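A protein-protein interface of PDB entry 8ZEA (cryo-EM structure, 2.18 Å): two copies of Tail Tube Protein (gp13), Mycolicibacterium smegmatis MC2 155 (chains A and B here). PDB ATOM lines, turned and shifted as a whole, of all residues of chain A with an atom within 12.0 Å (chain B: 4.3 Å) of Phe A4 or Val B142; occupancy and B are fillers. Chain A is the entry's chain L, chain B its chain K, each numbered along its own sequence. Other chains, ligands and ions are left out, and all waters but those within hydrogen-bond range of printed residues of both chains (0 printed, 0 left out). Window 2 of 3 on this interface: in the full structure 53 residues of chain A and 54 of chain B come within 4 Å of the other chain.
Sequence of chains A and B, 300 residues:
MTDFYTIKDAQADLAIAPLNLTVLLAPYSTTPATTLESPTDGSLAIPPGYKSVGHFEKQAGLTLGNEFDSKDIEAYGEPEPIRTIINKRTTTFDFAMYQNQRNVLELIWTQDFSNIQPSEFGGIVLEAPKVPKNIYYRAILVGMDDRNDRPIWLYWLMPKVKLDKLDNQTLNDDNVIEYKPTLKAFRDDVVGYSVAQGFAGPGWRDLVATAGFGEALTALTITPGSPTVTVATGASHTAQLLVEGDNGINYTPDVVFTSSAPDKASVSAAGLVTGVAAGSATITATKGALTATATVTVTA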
ATOM      1  N   THR A   2     -18.513  -3.602  -9.152  1.00  0.00           N
ATOM      2  CA  THR A   2     -18.954  -4.425  -8.033  1.00  0.00           C
ATOM      3  C   THR A   2     -18.388  -5.836  -8.139  1.00  0.00           C
ATOM      4  O   THR A   2     -18.605  -6.528  -9.134  1.00  0.00           O
ATOM      5  CB  THR A   2     -20.489  -4.506  -7.958  1.00  0.00           C
ATOM      6  OG1 THR A   2     -21.046  -3.197  -8.135  1.00  0.00           O
ATOM      7  CG2 THR A   2     -20.923  -5.048  -6.610  1.00  0.00           C
ATOM      8  N   ASP A   3     -17.662  -6.261  -7.111  1.00  0.00           N
ATOM      9  CA  ASP A   3     -17.083  -7.592  -7.095  1.00  0.00           C
ATOM     10  C   ASP A   3     -18.117  -8.623  -6.643  1.00  0.00           C
ATOM     11  O   ASP A   3     -19.226  -8.293  -6.221  1.00  0.00           O
ATOM     12  CB  ASP A   3     -15.850  -7.634  -6.193  1.00  0.00           C
ATOM     13  CG  ASP A   3     -16.194  -7.476  -4.731  1.00  0.00           C
ATOM     14  OD1 ASP A   3     -17.036  -6.616  -4.411  1.00  0.00           O
ATOM     15  OD2 ASP A   3     -15.628  -8.213  -3.900  1.00  0.00           O
ATOM     16  N   PHE A   4     -17.727  -9.895  -6.744  1.00  0.00           N
ATOM     17  CA  PHE A   4     -18.635 -10.994  -6.433  1.00  0.00           C
ATOM     18  C   PHE A   4     -19.070 -10.969  -4.973  1.00  0.00           C
ATOM     19  O   PHE A   4     -20.241 -11.212  -4.664  1.00  0.00           O
ATOM     20  CB  PHE A   4     -17.958 -12.322  -6.772  1.00  0.00           C
ATOM     21  CG  PHE A   4     -18.903 -13.482  -6.869  1.00  0.00           C
ATOM     22  CD1 PHE A   4     -19.518 -13.794  -8.069  1.00  0.00           C
ATOM     23  CD2 PHE A   4     -19.167 -14.270  -5.762  1.00  0.00           C
ATOM     24  CE1 PHE A   4     -20.381 -14.867  -8.161  1.00  0.00           C
ATOM     25  CE2 PHE A   4     -20.034 -15.342  -5.849  1.00  0.00           C
ATOM     26  CZ  PHE A   4     -20.638 -15.641  -7.050  1.00  0.00           C
ATOM     27  N   TYR A   5     -18.136 -10.680  -4.064  1.00  0.00           N
ATOM     28  CA  TYR A   5     -18.451 -10.682  -2.638  1.00  0.00           C
ATOM     29  C   TYR A   5     -19.498  -9.630  -2.293  1.00  0.00           C
ATOM     30  O   TYR A   5     -20.393  -9.880  -1.478  1.00  0.00           O
ATOM     31  CB  TYR A   5     -17.171 -10.465  -1.828  1.00  0.00           C
ATOM     32  CG  TYR A   5     -17.393 -10.169  -0.362  1.00  0.00           C
ATOM     33  CD1 TYR A   5     -17.502  -8.860   0.094  1.00  0.00           C
ATOM     34  CD2 TYR A   5     -17.484 -11.196   0.569  1.00  0.00           C
ATOM     35  CE1 TYR A   5     -17.706  -8.583   1.428  1.00  0.00           C
ATOM     36  CE2 TYR A   5     -17.687 -10.929   1.909  1.00  0.00           C
ATOM     37  CZ  TYR A   5     -17.796  -9.620   2.332  1.00  0.00           C
ATOM     38  OH  TYR A   5     -17.997  -9.341   3.665  1.00  0.00           O
ATOM     39  N   THR A   6     -19.396  -8.441  -2.889  1.00  0.00           N
ATOM     40  CA  THR A   6     -20.382  -7.398  -2.629  1.00  0.00           C
ATOM     41  C   THR A   6     -21.755  -7.787  -3.160  1.00  0.00           C
ATOM     42  O   THR A   6     -22.774  -7.524  -2.514  1.00  0.00           O
ATOM     43  CB  THR A   6     -19.928  -6.075  -3.243  1.00  0.00           C
ATOM     44  OG1 THR A   6     -18.592  -5.784  -2.820  1.00  0.00           O
ATOM     45  CG2 THR A   6     -20.847  -4.943  -2.818  1.00  0.00           C
ATOM     46  N   ILE A   7     -21.800  -8.407  -4.340  1.00  0.00           N
ATOM     47  CA  ILE A   7     -23.070  -8.847  -4.906  1.00  0.00           C
ATOM     48  C   ILE A   7     -23.702  -9.920  -4.027  1.00  0.00           C
ATOM     49  O   ILE A   7     -24.917  -9.918  -3.802  1.00  0.00           O
ATOM     50  CB  ILE A   7     -22.863  -9.338  -6.351  1.00  0.00           C
ATOM     51  CG1 ILE A   7     -22.597  -8.158  -7.284  1.00  0.00           C
ATOM     52  CG2 ILE A   7     -24.072 -10.116  -6.837  1.00  0.00           C
ATOM     53  CD1 ILE A   7     -21.825  -8.525  -8.526  1.00  0.00           C
ATOM     54  N   LYS A   8     -22.889 -10.843  -3.510  1.00  0.00           N
ATOM     55  CA  LYS A   8     -23.419 -11.930  -2.693  1.00  0.00           C
ATOM     56  C   LYS A   8     -24.076 -11.409  -1.418  1.00  0.00           C
ATOM     57  O   LYS A   8     -25.124 -11.914  -1.006  1.00  0.00           O
ATOM     58  CB  LYS A   8     -22.311 -12.927  -2.362  1.00  0.00           C
ATOM     59  CG  LYS A   8     -22.744 -14.030  -1.419  1.00  0.00           C
ATOM     60  CD  LYS A   8     -22.332 -15.396  -1.918  1.00  0.00           C
ATOM     61  CE  LYS A   8     -23.093 -16.489  -1.195  1.00  0.00           C
ATOM     62  NZ  LYS A   8     -22.562 -17.831  -1.516  1.00  0.00           N
ATOM     63  N   ASP A   9     -23.466 -10.410  -0.774  1.00  0.00           N
ATOM     64  CA  ASP A   9     -24.059  -9.727   0.381  1.00  0.00           C
ATOM     65  C   ASP A   9     -24.481 -10.714   1.468  1.00  0.00           C
ATOM     66  O   ASP A   9     -25.564 -10.612   2.047  1.00  0.00           O
ATOM     67  CB  ASP A   9     -25.243  -8.858  -0.048  1.00  0.00           C
ATOM     68  CG  ASP A   9     -25.632  -7.837   1.007  1.00  0.00           C
ATOM     69  OD1 ASP A   9     -24.739  -7.129   1.517  1.00  0.00           O
ATOM     70  OD2 ASP A   9     -26.834  -7.756   1.338  1.00  0.00           O
ATOM     71  N   ALA A  10     -23.623 -11.688   1.742  1.00  0.00           N
ATOM     72  CA  ALA A  10     -23.973 -12.732   2.691  1.00  0.00           C
ATOM     73  C   ALA A  10     -23.889 -12.217   4.123  1.00  0.00           C
ATOM     74  O   ALA A  10     -22.946 -11.514   4.494  1.00  0.00           O
ATOM     75  CB  ALA A  10     -23.058 -13.937   2.505  1.00  0.00           C
ATOM     76  N   GLN A  11     -24.890 -12.569   4.926  1.00  0.00           N
ATOM     77  CA  GLN A  11     -24.966 -12.189   6.335  1.00  0.00           C
ATOM     78  C   GLN A  11     -25.012 -13.467   7.167  1.00  0.00           C
ATOM     79  O   GLN A  11     -26.073 -14.079   7.316  1.00  0.00           O
ATOM     80  CB  GLN A  11     -26.186 -11.314   6.612  1.00  0.00           C
ATOM     81  CG  GLN A  11     -26.427 -10.211   5.600  1.00  0.00           C
ATOM     82  CD  GLN A  11     -25.406  -9.098   5.698  1.00  0.00           C
ATOM     83  OE1 GLN A  11     -25.252  -8.473   6.745  1.00  0.00           O
ATOM     84  NE2 GLN A  11     -24.704  -8.842   4.602  1.00  0.00           N
ATOM     85  N   ASN B  20     -17.335 -19.983  -6.070  1.00  0.00           N
ATOM     86  CA  ASN B  20     -18.357 -19.270  -5.327  1.00  0.00           C
ATOM     87  C   ASN B  20     -19.593 -19.122  -6.199  1.00  0.00           C
ATOM     88  O   ASN B  20     -19.515 -19.095  -7.429  1.00  0.00           O
ATOM     89  CB  ASN B  20     -17.865 -17.898  -4.855  1.00  0.00           C
ATOM     90  CG  ASN B  20     -18.462 -17.502  -3.520  1.00  0.00           C
ATOM     91  OD1 ASN B  20     -19.394 -18.140  -3.032  1.00  0.00           O
ATOM     92  ND2 ASN B  20     -17.926 -16.449  -2.922  1.00  0.00           N
ATOM     93  N   LEU B  21     -20.743 -19.047  -5.542  1.00  0.00           N
ATOM     94  CA  LEU B  21     -22.024 -19.039  -6.226  1.00  0.00           C
ATOM     95  C   LEU B  21     -23.001 -18.196  -5.426  1.00  0.00           C
ATOM     96  O   LEU B  21     -23.024 -18.264  -4.195  1.00  0.00           O
ATOM     97  CB  LEU B  21     -22.555 -20.465  -6.397  1.00  0.00           C
ATOM     98  CG  LEU B  21     -23.803 -20.719  -7.239  1.00  0.00           C
ATOM     99  CD1 LEU B  21     -23.611 -20.235  -8.662  1.00  0.00           C
ATOM    100  CD2 LEU B  21     -24.134 -22.200  -7.212  1.00  0.00           C
ATOM    101  N   THR B  22     -23.797 -17.399  -6.127  1.00  0.00           N
ATOM    102  CA  THR B  22     -24.830 -16.596  -5.494  1.00  0.00           C
ATOM    103  C   THR B  22     -26.113 -16.686  -6.306  1.00  0.00           C
ATOM    104  O   THR B  22     -26.082 -16.759  -7.536  1.00  0.00           O
ATOM    105  CB  THR B  22     -24.385 -15.130  -5.323  1.00  0.00           C
ATOM    106  OG1 THR B  22     -25.437 -14.360  -4.730  1.00  0.00           O
ATOM    107  CG2 THR B  22     -23.997 -14.519  -6.631  1.00  0.00           C
ATOM    108  N   LEU B  24     -29.668 -14.700  -6.950  1.00  0.00           N
ATOM    109  CA  LEU B  24     -30.345 -13.423  -6.801  1.00  0.00           C
ATOM    110  C   LEU B  24     -31.767 -13.552  -7.314  1.00  0.00           C
ATOM    111  O   LEU B  24     -32.002 -14.158  -8.363  1.00  0.00           O
ATOM    112  CB  LEU B  24     -29.612 -12.306  -7.542  1.00  0.00           C
ATOM    113  CG  LEU B  24     -28.223 -11.988  -6.993  1.00  0.00           C
ATOM    114  CD1 LEU B  24     -27.160 -12.672  -7.836  1.00  0.00           C
ATOM    115  CD2 LEU B  24     -27.988 -10.494  -6.893  1.00  0.00           C
ATOM    116  N   LEU B  36     -25.062 -10.204 -17.839  1.00  0.00           N
ATOM    117  CA  LEU B  36     -24.436  -9.743 -16.611  1.00  0.00           C
ATOM    118  C   LEU B  36     -23.168  -8.940 -16.865  1.00  0.00           C
ATOM    119  O   LEU B  36     -22.546  -8.472 -15.910  1.00  0.00           O
ATOM    120  CB  LEU B  36     -24.129 -10.935 -15.699  1.00  0.00           C
ATOM    121  CG  LEU B  36     -25.331 -11.743 -15.203  1.00  0.00           C
ATOM    122  CD1 LEU B  36     -24.946 -12.605 -14.016  1.00  0.00           C
ATOM    123  CD2 LEU B  36     -26.504 -10.839 -14.854  1.00  0.00           C
ATOM    124  N   LEU B  44     -18.719  -7.435 -13.908  1.00  0.00           N
ATOM    125  CA  LEU B  44     -19.996  -7.995 -13.489  1.00  0.00           C
ATOM    126  C   LEU B  44     -20.960  -6.880 -13.100  1.00  0.00           C
ATOM    127  O   LEU B  44     -20.617  -5.996 -12.311  1.00  0.00           O
ATOM    128  CB  LEU B  44     -19.784  -8.954 -12.320  1.00  0.00           C
ATOM    129  CG  LEU B  44     -20.768 -10.115 -12.184  1.00  0.00           C
ATOM    130  CD1 LEU B  44     -20.922 -10.849 -13.503  1.00  0.00           C
ATOM    131  CD2 LEU B  44     -20.302 -11.062 -11.096  1.00  0.00           C
ATOM    132  N   ILE B 140     -31.298 -14.979 -11.047  1.00  0.00           N
ATOM    133  CA  ILE B 140     -29.948 -15.050 -11.589  1.00  0.00           C
ATOM    134  C   ILE B 140     -29.145 -16.000 -10.712  1.00  0.00           C
ATOM    135  O   ILE B 140     -29.069 -15.813  -9.494  1.00  0.00           O
ATOM    136  CB  ILE B 140     -29.274 -13.667 -11.645  1.00  0.00           C
ATOM    137  CG1 ILE B 140     -29.987 -12.749 -12.640  1.00  0.00           C
ATOM    138  CG2 ILE B 140     -27.804 -13.806 -12.010  1.00  0.00           C
ATOM    139  CD1 ILE B 140     -29.546 -11.307 -12.550  1.00  0.00           C
ATOM    140  N   LEU B 141     -28.560 -17.017 -11.325  1.00  0.00           N
ATOM    141  CA  LEU B 141     -27.587 -17.878 -10.666  1.00  0.00           C
ATOM    142  C   LEU B 141     -26.243 -17.597 -11.313  1.00  0.00           C
ATOM    143  O   LEU B 141     -26.004 -18.016 -12.446  1.00  0.00           O
ATOM    144  CB  LEU B 141     -27.951 -19.354 -10.794  1.00  0.00           C
ATOM    145  CG  LEU B 141     -29.413 -19.793 -10.734  1.00  0.00           C
ATOM    146  CD1 LEU B 141     -29.501 -21.308 -10.833  1.00  0.00           C
ATOM    147  CD2 LEU B 141     -30.081 -19.302  -9.467  1.00  0.00           C
ATOM    148  N   VAL B 142     -25.369 -16.890 -10.609  1.00  0.00           N
ATOM    149  CA  VAL B 142     -24.064 -16.526 -11.143  1.00  0.00           C
ATOM    150  C   VAL B 142     -22.979 -17.110 -10.250  1.00  0.00           C
ATOM    151  O   VAL B 142     -23.005 -16.934  -9.026  1.00  0.00           O
ATOM    152  CB  VAL B 142     -23.916 -15.000 -11.313  1.00  0.00           C
ATOM    153  CG1 VAL B 142     -24.225 -14.267 -10.034  1.00  0.00           C
ATOM    154  CG2 VAL B 142     -22.518 -14.653 -11.802  1.00  0.00           C
ATOM    155  N   GLY B 143     -22.048 -17.826 -10.865  1.00  0.00           N
ATOM    156  CA  GLY B 143     -20.919 -18.395 -10.164  1.00  0.00           C
ATOM    157  C   GLY B 143     -19.617 -17.777 -10.616  1.00  0.00           C
ATOM    158  O   GLY B 143     -19.560 -17.135 -11.666  1.00  0.00           O
ATOM    159  N   MET B 144     -18.563 -17.951  -9.830  1.00  0.00           N
ATOM    160  CA  MET B 144     -17.261 -17.390 -10.147  1.00  0.00           C
ATOM    161  C   MET B 144     -16.205 -18.482 -10.092  1.00  0.00           C
ATOM    162  O   MET B 144     -16.171 -19.277  -9.148  1.00  0.00           O
ATOM    163  CB  MET B 144     -16.903 -16.251  -9.190  1.00  0.00           C
ATOM    164  CG  MET B 144     -15.716 -15.422  -9.647  1.00  0.00           C
ATOM    165  SD  MET B 144     -15.300 -14.071  -8.530  1.00  0.00           S
ATOM    166  CE  MET B 144     -15.350 -14.898  -6.946  1.00  0.00           C
ATOM    167  N   LEU B 154     -19.696 -17.653 -14.780  1.00  0.00           N
ATOM    168  CA  LEU B 154     -20.688 -18.493 -15.429  1.00  0.00           C
ATOM    169  C   LEU B 154     -22.020 -18.259 -14.737  1.00  0.00           C
ATOM    170  O   LEU B 154     -22.085 -18.226 -13.506  1.00  0.00           O
ATOM    171  CB  LEU B 154     -20.285 -19.970 -15.381  1.00  0.00           C
ATOM    172  CG  LEU B 154     -20.360 -20.751 -14.067  1.00  0.00           C
ATOM    173  CD1 LEU B 154     -20.280 -22.232 -14.353  1.00  0.00           C
ATOM    174  CD2 LEU B 154     -19.263 -20.341 -13.092  1.00  0.00           C
ATOM    175  N   TYR B 155     -23.072 -18.054 -15.520  1.00  0.00           N
ATOM    176  CA  TYR B 155     -24.351 -17.720 -14.923  1.00  0.00           C
ATOM    177  C   TYR B 155     -25.503 -18.303 -15.722  1.00  0.00           C
ATOM    178  O   TYR B 155     -25.364 -18.687 -16.885  1.00  0.00           O
ATOM    179  CB  TYR B 155     -24.530 -16.204 -14.764  1.00  0.00           C
ATOM    180  CG  TYR B 155     -24.385 -15.381 -16.020  1.00  0.00           C
ATOM    181  CD1 TYR B 155     -23.136 -14.981 -16.469  1.00  0.00           C
ATOM    182  CD2 TYR B 155     -25.502 -14.967 -16.731  1.00  0.00           C
ATOM    183  CE1 TYR B 155     -23.001 -14.210 -17.599  1.00  0.00           C
ATOM    184  CE2 TYR B 155     -25.378 -14.194 -17.859  1.00  0.00           C
ATOM    185  CZ  TYR B 155     -24.125 -13.818 -18.290  1.00  0.00           C
ATOM    186  OH  TYR B 155     -23.999 -13.049 -19.418  1.00  0.00           O
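Printed residues of chain A that touch a printed residue of chain B: Thr A2, Phe A4, Ile A7 and Lys A8. Hydrophobic or aromatic side chains of chain A within 4 Å of the printed part of chain B: Phe A4 and Ile A7. Along chain A the printed residues that touch a printed residue of chain B span positions 2 to 8. Printed residues of chain B that touch a printed residue of chain A: Asn B20, Leu B21, Thr B22, Leu B24, Leu B44, Val B142, Gly B143 and Met B144.
The backbone carbonyl oxygen (O) of Asn B20 is in hydrogen-bond range of the backbone NH (N) of Met B144 (2.8 Å). The backbone NH of Thr B22 sits at hydrogen-bond distance from the backbone carbonyl oxygen of Val B142 (3.0 Å). The backbone carbonyl oxygen (O) of Ile B140 lies within hydrogen-bond range of the backbone NH (N) of Leu B24, at 2.8 Å. The backbone NH of Gly B143 sits at hydrogen-bond distance from the backbone carbonyl oxygen of Leu B154 (2.7 Å).
Among the printed residues, pairs that only touch across the chains: Phe A4 with Val B142, Phe A4 with Asn B20, Lys A8 with Asn B20, Phe A4 with Thr B22, Phe A4 with Met B144, Phe A4 with Leu B21, Lys A8 with Thr B22, Thr A2 with Leu B44, Phe A4 with Gly B143, Ile A7 with Leu B44 and Ile A7 with Leu B24.
Printed residues of chain B within 4 Å of Thr A2: Leu B44. Phe A4 touches six residues of chain B. Tyr A5 touches none of the printed residues of chain B. Of the printed residues of chain B, Ile A7 touches Leu B24 and Leu B44. Of the printed residues of chain A, Leu B21 touches Phe A4 and Lys A8. Leu B24 touches one residue of chain A. No residue of chain A comes within 4 Å of Leu B36. No residue of chain A comes within 4 Å of Ile B140. No residue of chain A comes within 4 Å of Leu B141. Val B142 touches one residue of chain A. Of the printed residues of chain A, Gly B143 touches Phe A4. Met B144 touches just one residue of chain A: Phe A4 (3.6 Å). No residue of chain A comes within 4 Å of Leu B154. No residue of chain A comes within 4 Å of Tyr B155. The nearest residue of chain B that does not touch Phe A4 is Leu B44 (4.2 Å).
No position is printed for both chains. Of the 12 pairs that touch across the chains among the printed residues, none has its exchanged pair printed and touching as well.
O of Leu B21 lies within hydrogen-bond range of NZ of Lys A8, 2.8 Å away.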
